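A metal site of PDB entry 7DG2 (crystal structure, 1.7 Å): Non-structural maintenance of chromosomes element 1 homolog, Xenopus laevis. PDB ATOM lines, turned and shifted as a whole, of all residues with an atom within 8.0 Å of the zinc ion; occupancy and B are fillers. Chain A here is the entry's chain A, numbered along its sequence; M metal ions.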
ATOM      1  N   LEU A 196     -13.581   1.338  -2.151  1.00  0.00           N
ATOM      2  CA  LEU A 196     -12.792   2.237  -1.334  1.00  0.00           C
ATOM      3  C   LEU A 196     -13.218   3.683  -1.570  1.00  0.00           C
ATOM      4  O   LEU A 196     -13.486   4.070  -2.711  1.00  0.00           O
ATOM      5  CB  LEU A 196     -11.304   2.102  -1.642  1.00  0.00           C
ATOM      6  CG  LEU A 196     -10.666   0.733  -1.395  1.00  0.00           C
ATOM      7  CD1 LEU A 196      -9.335   0.658  -2.110  1.00  0.00           C
ATOM      8  CD2 LEU A 196     -10.513   0.511   0.105  1.00  0.00           C
ATOM      9  N   CYS A 197     -13.271   4.473  -0.504  1.00  0.00           N
ATOM     10  CA  CYS A 197     -13.340   5.907  -0.692  1.00  0.00           C
ATOM     11  C   CYS A 197     -12.065   6.384  -1.362  1.00  0.00           C
ATOM     12  O   CYS A 197     -10.965   6.066  -0.912  1.00  0.00           O
ATOM     13  CB  CYS A 197     -13.538   6.635   0.641  1.00  0.00           C
ATOM     14  SG  CYS A 197     -13.610   8.441   0.422  1.00  0.00           S
ATOM     15  N   GLU A 198     -12.209   7.118  -2.463  1.00  0.00           N
ATOM     16  CA  GLU A 198     -11.007   7.554  -3.155  1.00  0.00           C
ATOM     17  C   GLU A 198     -10.394   8.780  -2.517  1.00  0.00           C
ATOM     18  O   GLU A 198      -9.268   9.156  -2.872  1.00  0.00           O
ATOM     19  CB  GLU A 198     -11.316   7.784  -4.632  1.00  0.00           C
ATOM     20  CG  GLU A 198     -11.920   6.536  -5.276  1.00  0.00           C
ATOM     21  CD  GLU A 198     -11.928   6.587  -6.785  1.00  0.00           C
ATOM     22  OE1 GLU A 198     -11.417   5.640  -7.415  1.00  0.00           O
ATOM     23  OE2 GLU A 198     -12.453   7.569  -7.348  1.00  0.00           O
ATOM     24  N   ASN A 199     -11.090   9.403  -1.570  1.00  0.00           N
ATOM     25  CA  ASN A 199     -10.529  10.522  -0.823  1.00  0.00           C
ATOM     26  C   ASN A 199      -9.810  10.067   0.439  1.00  0.00           C
ATOM     27  O   ASN A 199      -8.650  10.445   0.657  1.00  0.00           O
ATOM     28  CB  ASN A 199     -11.617  11.537  -0.472  1.00  0.00           C
ATOM     29  CG  ASN A 199     -11.075  12.714   0.302  1.00  0.00           C
ATOM     30  OD1 ASN A 199     -10.220  13.454  -0.190  1.00  0.00           O
ATOM     31  ND2 ASN A 199     -11.564  12.887   1.529  1.00  0.00           N
ATOM     32  N   CYS A 200     -10.458   9.265   1.289  1.00  0.00           N
ATOM     33  CA  CYS A 200      -9.877   8.888   2.579  1.00  0.00           C
ATOM     34  C   CYS A 200      -9.514   7.412   2.688  1.00  0.00           C
ATOM     35  O   CYS A 200      -8.895   7.024   3.691  1.00  0.00           O
ATOM     36  CB  CYS A 200     -10.823   9.241   3.731  1.00  0.00           C
ATOM     37  SG  CYS A 200     -12.196   8.094   3.938  1.00  0.00           S
ATOM     38  N   GLY A 201      -9.892   6.584   1.724  1.00  0.00           N
ATOM     39  CA  GLY A 201      -9.408   5.211   1.678  1.00  0.00           C
ATOM     40  C   GLY A 201     -10.196   4.178   2.474  1.00  0.00           C
ATOM     41  O   GLY A 201      -9.799   3.004   2.470  1.00  0.00           O
ATOM     42  N   ILE A 202     -11.271   4.563   3.152  1.00  0.00           N
ATOM     43  CA  ILE A 202     -11.967   3.568   3.972  1.00  0.00           C
ATOM     44  C   ILE A 202     -12.671   2.565   3.067  1.00  0.00           C
ATOM     45  O   ILE A 202     -13.114   2.918   1.973  1.00  0.00           O
ATOM     46  CB  ILE A 202     -12.972   4.208   4.951  1.00  0.00           C
ATOM     47  CG1 ILE A 202     -14.062   4.974   4.208  1.00  0.00           C
ATOM     48  CG2 ILE A 202     -12.241   5.051   6.006  1.00  0.00           C
ATOM     49  CD1 ILE A 202     -15.378   4.222   4.107  1.00  0.00           C
ATOM     50  N   PRO A 203     -12.776   1.315   3.495  1.00  0.00           N
ATOM     51  CA  PRO A 203     -13.379   0.291   2.643  1.00  0.00           C
ATOM     52  C   PRO A 203     -14.802  -0.065   3.069  1.00  0.00           C
ATOM     53  O   PRO A 203     -15.141   0.017   4.254  1.00  0.00           O
ATOM     54  CB  PRO A 203     -12.438  -0.901   2.842  1.00  0.00           C
ATOM     55  CG  PRO A 203     -12.033  -0.778   4.298  1.00  0.00           C
ATOM     56  CD  PRO A 203     -12.042   0.715   4.633  1.00  0.00           C
ATOM     57  N   THR A 220     -22.688   9.718   0.255  1.00  0.00           N
ATOM     58  CA  THR A 220     -21.455  10.287   0.766  1.00  0.00           C
ATOM     59  C   THR A 220     -20.744   9.296   1.664  1.00  0.00           C
ATOM     60  O   THR A 220     -21.374   8.446   2.315  1.00  0.00           O
ATOM     61  CB  THR A 220     -21.708  11.583   1.554  1.00  0.00           C
ATOM     62  OG1 THR A 220     -22.620  11.317   2.627  1.00  0.00           O
ATOM     63  CG2 THR A 220     -22.294  12.661   0.639  1.00  0.00           C
ATOM     64  N   CYS A 221     -19.420   9.417   1.709  1.00  0.00           N
ATOM     65  CA  CYS A 221     -18.579   8.518   2.504  1.00  0.00           C
ATOM     66  C   CYS A 221     -18.891   8.673   3.991  1.00  0.00           C
ATOM     67  O   CYS A 221     -18.901   9.801   4.501  1.00  0.00           O
ATOM     68  CB  CYS A 221     -17.108   8.824   2.236  1.00  0.00           C
ATOM     69  SG  CYS A 221     -15.938   8.035   3.387  1.00  0.00           S
ATOM     70  N   PRO A 222     -19.103   7.575   4.722  1.00  0.00           N
ATOM     71  CA  PRO A 222     -19.441   7.686   6.153  1.00  0.00           C
ATOM     72  C   PRO A 222     -18.294   8.210   7.013  1.00  0.00           C
ATOM     73  O   PRO A 222     -18.526   8.508   8.196  1.00  0.00           O
ATOM     74  CB  PRO A 222     -19.809   6.251   6.557  1.00  0.00           C
ATOM     75  CG  PRO A 222     -19.489   5.375   5.371  1.00  0.00           C
ATOM     76  CD  PRO A 222     -18.797   6.188   4.335  1.00  0.00           C
ATOM     77  N   ASN A 223     -17.081   8.331   6.464  1.00  0.00           N
ATOM     78  CA  ASN A 223     -15.918   8.759   7.223  1.00  0.00           C
ATOM     79  C   ASN A 223     -15.477  10.181   6.917  1.00  0.00           C
ATOM     80  O   ASN A 223     -15.142  10.924   7.835  1.00  0.00           O
ATOM     81  CB  ASN A 223     -14.747   7.802   6.961  1.00  0.00           C
ATOM     82  CG  ASN A 223     -13.536   8.098   7.832  1.00  0.00           C
ATOM     83  OD1 ASN A 223     -13.638   8.081   9.057  1.00  0.00           O
ATOM     84  ND2 ASN A 223     -12.395   8.359   7.202  1.00  0.00           N
ATOM     85  N   CYS A 224     -15.455  10.573   5.641  1.00  0.00           N
ATOM     86  CA  CYS A 224     -14.990  11.896   5.250  1.00  0.00           C
ATOM     87  C   CYS A 224     -16.064  12.736   4.577  1.00  0.00           C
ATOM     88  O   CYS A 224     -15.802  13.893   4.245  1.00  0.00           O
ATOM     89  CB  CYS A 224     -13.780  11.788   4.326  1.00  0.00           C
ATOM     90  SG  CYS A 224     -14.174  11.299   2.623  1.00  0.00           S
ATOM     91  N   ASN A 225     -17.263  12.184   4.353  1.00  0.00           N
ATOM     92  CA  ASN A 225     -18.424  12.870   3.789  1.00  0.00           C
ATOM     93  C   ASN A 225     -18.253  13.319   2.333  1.00  0.00           C
ATOM     94  O   ASN A 225     -19.124  14.022   1.814  1.00  0.00           O
ATOM     95  CB  ASN A 225     -18.842  14.074   4.639  1.00  0.00           C
ATOM     96  CG  ASN A 225     -19.252  13.674   6.033  1.00  0.00           C
ATOM     97  OD1 ASN A 225     -19.624  12.518   6.288  1.00  0.00           O
ATOM     98  ND2 ASN A 225     -19.194  14.616   6.966  1.00  0.00           N
ATOM     99  N   GLU A 226     -17.158  12.960   1.674  1.00  0.00           N
ATOM    100  CA  GLU A 226     -17.067  13.188   0.240  1.00  0.00           C
ATOM    101  C   GLU A 226     -18.064  12.306  -0.484  1.00  0.00           C
ATOM    102  O   GLU A 226     -18.424  11.217  -0.016  1.00  0.00           O
ATOM    103  CB  GLU A 226     -15.649  12.930  -0.272  1.00  0.00           C
ATOM    104  CG  GLU A 226     -14.594  13.902   0.235  1.00  0.00           C
ATOM    105  CD  GLU A 226     -14.967  15.357  -0.006  1.00  0.00           C
ATOM    106  OE1 GLU A 226     -15.593  15.968   0.888  1.00  0.00           O
ATOM    107  OE2 GLU A 226     -14.627  15.876  -1.092  1.00  0.00           O
ATOM    108  N   SER A 227     -18.556  12.774  -1.633  1.00  0.00           N
ATOM    109  CA  SER A 227     -19.541  11.991  -2.366  1.00  0.00           C
ATOM    110  C   SER A 227     -18.920  10.674  -2.810  1.00  0.00           C
ATOM    111  O   SER A 227     -17.753  10.614  -3.222  1.00  0.00           O
ATOM    112  CB  SER A 227     -20.069  12.779  -3.569  1.00  0.00           C
ATOM    113  OG  SER A 227     -19.017  13.181  -4.418  1.00  0.00           O
ATOM    114  N   TRP A 228     -19.705   9.605  -2.704  1.00  0.00           N
ATOM    115  CA  TRP A 228     -19.215   8.259  -3.007  1.00  0.00           C
ATOM    116  C   TRP A 228     -19.002   8.101  -4.512  1.00  0.00           C
ATOM    117  O   TRP A 228     -19.962   8.264  -5.287  1.00  0.00           O
ATOM    118  CB  TRP A 228     -20.200   7.219  -2.490  1.00  0.00           C
ATOM    119  CG  TRP A 228     -19.611   5.838  -2.331  1.00  0.00           C
ATOM    120  CD1 TRP A 228     -19.981   4.709  -3.002  1.00  0.00           C
ATOM    121  CD2 TRP A 228     -18.539   5.458  -1.456  1.00  0.00           C
ATOM    122  NE1 TRP A 228     -19.205   3.644  -2.590  1.00  0.00           N
ATOM    123  CE2 TRP A 228     -18.318   4.084  -1.642  1.00  0.00           C
ATOM    124  CE3 TRP A 228     -17.762   6.154  -0.534  1.00  0.00           C
ATOM    125  CZ2 TRP A 228     -17.336   3.388  -0.931  1.00  0.00           C
ATOM    126  CZ3 TRP A 228     -16.788   5.466   0.169  1.00  0.00           C
ATOM    127  CH2 TRP A 228     -16.584   4.095  -0.034  1.00  0.00           C
ATOM    128  N   PRO A 229     -17.797   7.776  -4.963  1.00  0.00           N
ATOM    129  CA  PRO A 229     -17.517   7.764  -6.408  1.00  0.00           C
ATOM    130  C   PRO A 229     -18.022   6.532  -7.142  1.00  0.00           C
ATOM    131  O   PRO A 229     -18.090   6.554  -8.382  1.00  0.00           O
ATOM    132  CB  PRO A 229     -15.987   7.833  -6.465  1.00  0.00           C
ATOM    133  CG  PRO A 229     -15.549   7.145  -5.210  1.00  0.00           C
ATOM    134  CD  PRO A 229     -16.589   7.493  -4.168  1.00  0.00           C
HETATM  135 ZN    ZN M   1     -13.969   8.951   2.711  1.00  0.00          ZN
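The zinc ion is bound by SG of Cys 221 (2.3 Å). The zinc ion is bound by SG of Cys 200 (2.3 Å). The zinc ion is bound by the side-chain sulfur (SG) of Cys 224, at 2.4 Å. The zinc ion is bound by SG of Cys 197 (2.4 Å). The zinc ion has four donor atoms within binding distance.
The backbone carbonyl oxygen of Cys 221 sits close to the side-chain amide oxygen of Asn 225 (3.3 Å). N of Cys 221 lies within hydrogen-bond range of O of Glu 226, 2.7 Å away. The backbone NH (N) of Ile 202 sits close to the side-chain sulfur (SG) of Cys 200. The side-chain sulfur (SG) of Cys 200 sits close to the side-chain amide nitrogen (ND2) of Asn 223 (3.3 Å). SG of Cys 224 sits close to ND2 of Asn 199, at 3.2 Å. N of Glu 226 sits close to SG of Cys 224 (3.5 Å). The backbone NH of Cys 197 is in hydrogen-bond range of the backbone carbonyl oxygen of Ile 202 (2.9 Å). The backbone NH (N) of Asn 199 lies close to the side-chain sulfur (SG) of Cys 197 (3.4 Å).
Of the 18 residues printed, 4 come within 4 Å of the zinc ion.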
